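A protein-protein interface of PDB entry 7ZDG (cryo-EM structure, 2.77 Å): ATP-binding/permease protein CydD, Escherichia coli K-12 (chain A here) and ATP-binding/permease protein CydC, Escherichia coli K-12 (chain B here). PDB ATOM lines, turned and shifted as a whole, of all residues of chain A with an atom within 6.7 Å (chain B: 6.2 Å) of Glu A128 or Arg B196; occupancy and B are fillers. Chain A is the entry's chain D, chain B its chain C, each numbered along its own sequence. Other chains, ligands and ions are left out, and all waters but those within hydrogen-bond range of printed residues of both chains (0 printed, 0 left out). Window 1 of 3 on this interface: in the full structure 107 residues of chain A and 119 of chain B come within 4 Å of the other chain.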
ATOM      1  N   ARG A  99      15.311 -30.948  38.793  1.00  0.00           N
ATOM      2  CA  ARG A  99      16.588 -30.938  38.093  1.00  0.00           C
ATOM      3  C   ARG A  99      17.736 -31.258  39.036  1.00  0.00           C
ATOM      4  O   ARG A  99      18.698 -31.924  38.649  1.00  0.00           O
ATOM      5  CB  ARG A  99      16.797 -29.588  37.420  1.00  0.00           C
ATOM      6  CG  ARG A  99      17.804 -29.610  36.313  1.00  0.00           C
ATOM      7  CD  ARG A  99      17.789 -28.318  35.551  1.00  0.00           C
ATOM      8  NE  ARG A  99      16.821 -28.341  34.466  1.00  0.00           N
ATOM      9  CZ  ARG A  99      15.870 -27.435  34.305  1.00  0.00           C
ATOM     10  NH1 ARG A  99      15.762 -26.434  35.157  1.00  0.00           N
ATOM     11  NH2 ARG A  99      15.029 -27.532  33.294  1.00  0.00           N
ATOM     12  N   GLY A 120      23.291 -36.097  24.384  1.00  0.00           N
ATOM     13  CA  GLY A 120      22.154 -35.324  23.929  1.00  0.00           C
ATOM     14  C   GLY A 120      20.836 -35.873  24.425  1.00  0.00           C
ATOM     15  O   GLY A 120      19.839 -35.151  24.471  1.00  0.00           O
ATOM     16  N   ALA A 123      20.483 -34.489  27.883  1.00  0.00           N
ATOM     17  CA  ALA A 123      20.070 -33.097  27.802  1.00  0.00           C
ATOM     18  C   ALA A 123      18.585 -32.975  27.517  1.00  0.00           C
ATOM     19  O   ALA A 123      17.956 -31.998  27.927  1.00  0.00           O
ATOM     20  CB  ALA A 123      20.883 -32.376  26.734  1.00  0.00           C
ATOM     21  N   THR A 124      18.011 -33.942  26.806  1.00  0.00           N
ATOM     22  CA  THR A 124      16.569 -33.959  26.618  1.00  0.00           C
ATOM     23  C   THR A 124      15.851 -34.182  27.938  1.00  0.00           C
ATOM     24  O   THR A 124      14.856 -33.514  28.234  1.00  0.00           O
ATOM     25  CB  THR A 124      16.190 -35.039  25.609  1.00  0.00           C
ATOM     26  OG1 THR A 124      16.604 -34.628  24.306  1.00  0.00           O
ATOM     27  CG2 THR A 124      14.701 -35.263  25.595  1.00  0.00           C
ATOM     28  N   LEU A 125      16.344 -35.117  28.747  1.00  0.00           N
ATOM     29  CA  LEU A 125      15.731 -35.375  30.041  1.00  0.00           C
ATOM     30  C   LEU A 125      15.854 -34.174  30.966  1.00  0.00           C
ATOM     31  O   LEU A 125      14.895 -33.807  31.648  1.00  0.00           O
ATOM     32  CB  LEU A 125      16.377 -36.595  30.683  1.00  0.00           C
ATOM     33  CG  LEU A 125      15.824 -37.035  32.032  1.00  0.00           C
ATOM     34  CD1 LEU A 125      14.492 -37.705  31.856  1.00  0.00           C
ATOM     35  CD2 LEU A 125      16.799 -37.937  32.724  1.00  0.00           C
ATOM     36  N   VAL A 126      17.025 -33.547  30.998  1.00  0.00           N
ATOM     37  CA  VAL A 126      17.292 -32.520  31.995  1.00  0.00           C
ATOM     38  C   VAL A 126      16.751 -31.171  31.551  1.00  0.00           C
ATOM     39  O   VAL A 126      16.217 -30.414  32.364  1.00  0.00           O
ATOM     40  CB  VAL A 126      18.799 -32.464  32.302  1.00  0.00           C
ATOM     41  CG1 VAL A 126      19.110 -31.333  33.252  1.00  0.00           C
ATOM     42  CG2 VAL A 126      19.264 -33.776  32.886  1.00  0.00           C
ATOM     43  N   LEU A 127      16.875 -30.829  30.270  1.00  0.00           N
ATOM     44  CA  LEU A 127      16.364 -29.535  29.828  1.00  0.00           C
ATOM     45  C   LEU A 127      14.922 -29.617  29.346  1.00  0.00           C
ATOM     46  O   LEU A 127      14.035 -28.995  29.930  1.00  0.00           O
ATOM     47  CB  LEU A 127      17.231 -28.940  28.713  1.00  0.00           C
ATOM     48  CG  LEU A 127      18.539 -28.216  29.008  1.00  0.00           C
ATOM     49  CD1 LEU A 127      19.641 -29.172  29.349  1.00  0.00           C
ATOM     50  CD2 LEU A 127      18.917 -27.342  27.845  1.00  0.00           C
ATOM     51  N   GLU A 128      14.673 -30.390  28.292  1.00  0.00           N
ATOM     52  CA  GLU A 128      13.391 -30.308  27.602  1.00  0.00           C
ATOM     53  C   GLU A 128      12.261 -30.883  28.441  1.00  0.00           C
ATOM     54  O   GLU A 128      11.200 -30.269  28.568  1.00  0.00           O
ATOM     55  CB  GLU A 128      13.477 -31.028  26.259  1.00  0.00           C
ATOM     56  CG  GLU A 128      13.896 -30.139  25.118  1.00  0.00           C
ATOM     57  CD  GLU A 128      15.351 -29.723  25.196  1.00  0.00           C
ATOM     58  OE1 GLU A 128      16.220 -30.606  25.318  1.00  0.00           O
ATOM     59  OE2 GLU A 128      15.626 -28.505  25.131  1.00  0.00           O
ATOM     60  N   GLN A 129      12.464 -32.064  29.014  1.00  0.00           N
ATOM     61  CA  GLN A 129      11.368 -32.752  29.676  1.00  0.00           C
ATOM     62  C   GLN A 129      11.090 -32.211  31.068  1.00  0.00           C
ATOM     63  O   GLN A 129       9.938 -32.209  31.500  1.00  0.00           O
ATOM     64  CB  GLN A 129      11.650 -34.246  29.725  1.00  0.00           C
ATOM     65  CG  GLN A 129      11.452 -34.897  28.389  1.00  0.00           C
ATOM     66  CD  GLN A 129      11.524 -36.382  28.458  1.00  0.00           C
ATOM     67  OE1 GLN A 129      12.508 -36.940  28.920  1.00  0.00           O
ATOM     68  NE2 GLN A 129      10.481 -37.043  27.992  1.00  0.00           N
ATOM     69  N   ILE A 130      12.108 -31.754  31.791  1.00  0.00           N
ATOM     70  CA  ILE A 130      11.833 -31.074  33.048  1.00  0.00           C
ATOM     71  C   ILE A 130      11.117 -29.759  32.785  1.00  0.00           C
ATOM     72  O   ILE A 130      10.226 -29.358  33.538  1.00  0.00           O
ATOM     73  CB  ILE A 130      13.128 -30.879  33.853  1.00  0.00           C
ATOM     74  CG1 ILE A 130      13.644 -32.223  34.349  1.00  0.00           C
ATOM     75  CG2 ILE A 130      12.891 -29.966  35.029  1.00  0.00           C
ATOM     76  CD1 ILE A 130      14.864 -32.123  35.186  1.00  0.00           C
ATOM     77  N   ASP A 131      11.472 -29.079  31.699  1.00  0.00           N
ATOM     78  CA  ASP A 131      10.804 -27.838  31.345  1.00  0.00           C
ATOM     79  C   ASP A 131       9.429 -28.062  30.739  1.00  0.00           C
ATOM     80  O   ASP A 131       8.623 -27.132  30.718  1.00  0.00           O
ATOM     81  CB  ASP A 131      11.666 -27.039  30.381  1.00  0.00           C
ATOM     82  CG  ASP A 131      12.559 -26.060  31.087  1.00  0.00           C
ATOM     83  OD1 ASP A 131      12.878 -26.288  32.267  1.00  0.00           O
ATOM     84  OD2 ASP A 131      12.938 -25.054  30.465  1.00  0.00           O
ATOM     85  N   ASP A 132       9.142 -29.263  30.239  1.00  0.00           N
ATOM     86  CA  ASP A 132       7.799 -29.570  29.764  1.00  0.00           C
ATOM     87  C   ASP A 132       6.807 -29.705  30.901  1.00  0.00           C
ATOM     88  O   ASP A 132       5.602 -29.748  30.650  1.00  0.00           O
ATOM     89  CB  ASP A 132       7.800 -30.853  28.939  1.00  0.00           C
ATOM     90  CG  ASP A 132       8.239 -30.628  27.513  1.00  0.00           C
ATOM     91  OD1 ASP A 132       8.422 -29.457  27.130  1.00  0.00           O
ATOM     92  OD2 ASP A 132       8.407 -31.616  26.772  1.00  0.00           O
ATOM     93  N   MET A 133       7.274 -29.770  32.140  1.00  0.00           N
ATOM     94  CA  MET A 133       6.372 -29.878  33.272  1.00  0.00           C
ATOM     95  C   MET A 133       5.962 -28.533  33.840  1.00  0.00           C
ATOM     96  O   MET A 133       5.162 -28.508  34.771  1.00  0.00           O
ATOM     97  CB  MET A 133       6.996 -30.692  34.400  1.00  0.00           C
ATOM     98  CG  MET A 133       7.237 -32.146  34.102  1.00  0.00           C
ATOM     99  SD  MET A 133       7.888 -32.916  35.578  1.00  0.00           S
ATOM    100  CE  MET A 133       9.538 -32.262  35.591  1.00  0.00           C
ATOM    101  N   ALA A 320       6.362 -36.027  29.953  1.00  0.00           N
ATOM    102  CA  ALA A 320       7.643 -35.786  30.600  1.00  0.00           C
ATOM    103  C   ALA A 320       7.775 -36.591  31.880  1.00  0.00           C
ATOM    104  O   ALA A 320       8.852 -37.108  32.182  1.00  0.00           O
ATOM    105  CB  ALA A 320       7.801 -34.300  30.889  1.00  0.00           C
ATOM    106  N   ASN B 191      18.121 -13.169  25.506  1.00  0.00           N
ATOM    107  CA  ASN B 191      18.867 -13.623  26.670  1.00  0.00           C
ATOM    108  C   ASN B 191      18.408 -15.007  27.097  1.00  0.00           C
ATOM    109  O   ASN B 191      19.158 -15.753  27.733  1.00  0.00           O
ATOM    110  CB  ASN B 191      18.697 -12.626  27.811  1.00  0.00           C
ATOM    111  CG  ASN B 191      19.692 -12.842  28.920  1.00  0.00           C
ATOM    112  OD1 ASN B 191      20.832 -13.231  28.679  1.00  0.00           O
ATOM    113  ND2 ASN B 191      19.269 -12.592  30.150  1.00  0.00           N
ATOM    114  N   LEU B 192      17.170 -15.362  26.760  1.00  0.00           N
ATOM    115  CA  LEU B 192      16.630 -16.667  27.119  1.00  0.00           C
ATOM    116  C   LEU B 192      17.204 -17.765  26.239  1.00  0.00           C
ATOM    117  O   LEU B 192      17.520 -18.855  26.722  1.00  0.00           O
ATOM    118  CB  LEU B 192      15.111 -16.622  27.003  1.00  0.00           C
ATOM    119  CG  LEU B 192      14.249 -17.637  27.719  1.00  0.00           C
ATOM    120  CD1 LEU B 192      14.538 -17.573  29.175  1.00  0.00           C
ATOM    121  CD2 LEU B 192      12.815 -17.282  27.464  1.00  0.00           C
ATOM    122  N   THR B 193      17.326 -17.505  24.939  1.00  0.00           N
ATOM    123  CA  THR B 193      17.923 -18.484  24.039  1.00  0.00           C
ATOM    124  C   THR B 193      19.413 -18.634  24.305  1.00  0.00           C
ATOM    125  O   THR B 193      19.959 -19.738  24.220  1.00  0.00           O
ATOM    126  CB  THR B 193      17.678 -18.077  22.588  1.00  0.00           C
ATOM    127  OG1 THR B 193      16.285 -18.193  22.291  1.00  0.00           O
ATOM    128  CG2 THR B 193      18.450 -18.972  21.643  1.00  0.00           C
ATOM    129  N   HIS B 194      20.084 -17.530  24.621  1.00  0.00           N
ATOM    130  CA  HIS B 194      21.509 -17.590  24.915  1.00  0.00           C
ATOM    131  C   HIS B 194      21.780 -18.388  26.180  1.00  0.00           C
ATOM    132  O   HIS B 194      22.728 -19.173  26.234  1.00  0.00           O
ATOM    133  CB  HIS B 194      22.070 -16.177  25.038  1.00  0.00           C
ATOM    134  CG  HIS B 194      23.436 -16.121  25.638  1.00  0.00           C
ATOM    135  ND1 HIS B 194      23.660 -15.739  26.941  1.00  0.00           N
ATOM    136  CD2 HIS B 194      24.650 -16.405  25.116  1.00  0.00           C
ATOM    137  CE1 HIS B 194      24.953 -15.792  27.198  1.00  0.00           C
ATOM    138  NE2 HIS B 194      25.577 -16.191  26.105  1.00  0.00           N
ATOM    139  N   LEU B 195      20.951 -18.204  27.206  1.00  0.00           N
ATOM    140  CA  LEU B 195      21.169 -18.877  28.480  1.00  0.00           C
ATOM    141  C   LEU B 195      20.768 -20.343  28.418  1.00  0.00           C
ATOM    142  O   LEU B 195      21.295 -21.164  29.173  1.00  0.00           O
ATOM    143  CB  LEU B 195      20.397 -18.158  29.577  1.00  0.00           C
ATOM    144  CG  LEU B 195      21.073 -16.929  30.164  1.00  0.00           C
ATOM    145  CD1 LEU B 195      20.142 -16.258  31.121  1.00  0.00           C
ATOM    146  CD2 LEU B 195      22.341 -17.321  30.862  1.00  0.00           C
ATOM    147  N   ARG B 196      19.819 -20.691  27.552  1.00  0.00           N
ATOM    148  CA  ARG B 196      19.459 -22.093  27.387  1.00  0.00           C
ATOM    149  C   ARG B 196      20.553 -22.861  26.664  1.00  0.00           C
ATOM    150  O   ARG B 196      20.853 -24.005  27.015  1.00  0.00           O
ATOM    151  CB  ARG B 196      18.144 -22.224  26.626  1.00  0.00           C
ATOM    152  CG  ARG B 196      17.695 -23.656  26.509  1.00  0.00           C
ATOM    153  CD  ARG B 196      17.009 -23.942  25.207  1.00  0.00           C
ATOM    154  NE  ARG B 196      17.006 -25.373  24.919  1.00  0.00           N
ATOM    155  CZ  ARG B 196      17.998 -26.012  24.302  1.00  0.00           C
ATOM    156  NH1 ARG B 196      17.918 -27.316  24.085  1.00  0.00           N
ATOM    157  NH2 ARG B 196      19.072 -25.350  23.895  1.00  0.00           N
ATOM    158  N   GLY B 197      21.143 -22.262  25.633  1.00  0.00           N
ATOM    159  CA  GLY B 197      22.213 -22.933  24.922  1.00  0.00           C
ATOM    160  C   GLY B 197      23.490 -23.000  25.731  1.00  0.00           C
ATOM    161  O   GLY B 197      24.279 -23.933  25.585  1.00  0.00           O
ATOM    162  N   GLN B 198      23.716 -22.005  26.586  1.00  0.00           N
ATOM    163  CA  GLN B 198      24.873 -22.034  27.467  1.00  0.00           C
ATOM    164  C   GLN B 198      24.721 -23.096  28.542  1.00  0.00           C
ATOM    165  O   GLN B 198      25.692 -23.770  28.894  1.00  0.00           O
ATOM    166  CB  GLN B 198      25.087 -20.663  28.095  1.00  0.00           C
ATOM    167  CG  GLN B 198      25.895 -20.700  29.362  1.00  0.00           C
ATOM    168  CD  GLN B 198      26.442 -19.350  29.737  1.00  0.00           C
ATOM    169  OE1 GLN B 198      26.941 -18.618  28.890  1.00  0.00           O
ATOM    170  NE2 GLN B 198      26.358 -19.011  31.014  1.00  0.00           N
ATOM    171  N   TYR B 199      23.516 -23.258  29.084  1.00  0.00           N
ATOM    172  CA  TYR B 199      23.282 -24.320  30.054  1.00  0.00           C
ATOM    173  C   TYR B 199      23.455 -25.691  29.422  1.00  0.00           C
ATOM    174  O   TYR B 199      24.019 -26.597  30.039  1.00  0.00           O
ATOM    175  CB  TYR B 199      21.887 -24.196  30.656  1.00  0.00           C
ATOM    176  CG  TYR B 199      21.620 -25.204  31.737  1.00  0.00           C
ATOM    177  CD1 TYR B 199      21.974 -24.945  33.038  1.00  0.00           C
ATOM    178  CD2 TYR B 199      21.029 -26.424  31.454  1.00  0.00           C
ATOM    179  CE1 TYR B 199      21.745 -25.851  34.024  1.00  0.00           C
ATOM    180  CE2 TYR B 199      20.800 -27.341  32.440  1.00  0.00           C
ATOM    181  CZ  TYR B 199      21.160 -27.044  33.724  1.00  0.00           C
ATOM    182  OH  TYR B 199      20.941 -27.944  34.729  1.00  0.00           O
ATOM    183  N   ARG B 200      22.953 -25.872  28.202  1.00  0.00           N
ATOM    184  CA  ARG B 200      23.082 -27.165  27.543  1.00  0.00           C
ATOM    185  C   ARG B 200      24.536 -27.493  27.263  1.00  0.00           C
ATOM    186  O   ARG B 200      24.938 -28.658  27.306  1.00  0.00           O
ATOM    187  CB  ARG B 200      22.278 -27.181  26.248  1.00  0.00           C
ATOM    188  CG  ARG B 200      22.173 -28.549  25.640  1.00  0.00           C
ATOM    189  CD  ARG B 200      21.613 -28.509  24.248  1.00  0.00           C
ATOM    190  NE  ARG B 200      21.185 -29.832  23.809  1.00  0.00           N
ATOM    191  CZ  ARG B 200      22.005 -30.783  23.367  1.00  0.00           C
ATOM    192  NH1 ARG B 200      21.517 -31.956  22.995  1.00  0.00           N
ATOM    193  NH2 ARG B 200      23.308 -30.567  23.295  1.00  0.00           N
ATOM    194  N   GLN B 201      25.335 -26.479  26.952  1.00  0.00           N
ATOM    195  CA  GLN B 201      26.753 -26.694  26.707  1.00  0.00           C
ATOM    196  C   GLN B 201      27.487 -27.058  27.989  1.00  0.00           C
ATOM    197  O   GLN B 201      28.360 -27.929  27.981  1.00  0.00           O
ATOM    198  CB  GLN B 201      27.353 -25.448  26.072  1.00  0.00           C
ATOM    199  CG  GLN B 201      28.845 -25.471  25.953  1.00  0.00           C
ATOM    200  CD  GLN B 201      29.393 -24.155  25.472  1.00  0.00           C
ATOM    201  OE1 GLN B 201      28.655 -23.182  25.319  1.00  0.00           O
ATOM    202  NE2 GLN B 201      30.697 -24.111  25.230  1.00  0.00           N
ATOM    203  N   TRP B 233      19.317 -18.482  33.969  1.00  0.00           N
ATOM    204  CA  TRP B 233      18.330 -18.923  32.995  1.00  0.00           C
ATOM    205  C   TRP B 233      16.919 -18.849  33.561  1.00  0.00           C
ATOM    206  O   TRP B 233      15.978 -18.482  32.856  1.00  0.00           O
ATOM    207  CB  TRP B 233      18.675 -20.339  32.553  1.00  0.00           C
ATOM    208  CG  TRP B 233      17.804 -20.913  31.524  1.00  0.00           C
ATOM    209  CD1 TRP B 233      17.042 -20.246  30.626  1.00  0.00           C
ATOM    210  CD2 TRP B 233      17.608 -22.299  31.269  1.00  0.00           C
ATOM    211  NE1 TRP B 233      16.372 -21.130  29.828  1.00  0.00           N
ATOM    212  CE2 TRP B 233      16.705 -22.401  30.205  1.00  0.00           C
ATOM    213  CE3 TRP B 233      18.107 -23.469  31.846  1.00  0.00           C
ATOM    214  CZ2 TRP B 233      16.288 -23.623  29.702  1.00  0.00           C
ATOM    215  CZ3 TRP B 233      17.695 -24.676  31.346  1.00  0.00           C
ATOM    216  CH2 TRP B 233      16.795 -24.747  30.283  1.00  0.00           C
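The guanidinium group of Arg A99 lies within hydrogen-bond range of the backbone carbonyl oxygen of Val A126 (3.0 Å). The guanidinium group (NH2) of Arg A99 is in salt-bridge range of the side-chain carboxylate (OD1) of Asp A131 (2.7 Å). The backbone carbonyl oxygen (O) of Gly A120 lies within hydrogen-bond range of the side-chain hydroxyl (OG1) of Thr A124.
Among the printed residues, pairs that only touch across the chains: Arg A99 with Tyr B199, Gly A120 with Arg B200, Ala A123 with Arg B200, Leu A127 with Arg B196, Leu A127 with Tyr B199, Leu A127 with Arg B200 and Asp A131 with Trp B233.
Glu A128 touches just one residue of chain B: Arg B196. Printed residues of chain A within 4 Å of Arg B196: Leu A127 (3.9 Å) and Glu A128 (2.8 Å). Printed residues of chain B within 4 Å of Ala A123: Arg B200 (3.8 Å). Printed residues of chain A within 4 Å of Arg B200: Gly A120 (3.6 Å), Ala A123 (3.8 Å) and Leu A127 (3.7 Å). Met A133 touches none of the printed residues of chain B. Asn B191 touches none of the printed residues of chain A. The nearest residue of chain A that does not touch Arg B196 is Ala A123 (6.1 Å).
Of the 14 printed residues of chain A, 6 touch a printed residue of chain B. Of the 12 printed residues of chain B, 4 touch a printed residue of chain A. Among the printed residues, Asp or Glu carboxylates within 4 Å of a Lys or Arg side-chain nitrogen of the other chain: Glu A128 with Arg B196 (2.8 Å).
The guanidinium group of Arg B196 is in salt-bridge range of the side-chain carboxylate of Glu A128, 2.8 Å away.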
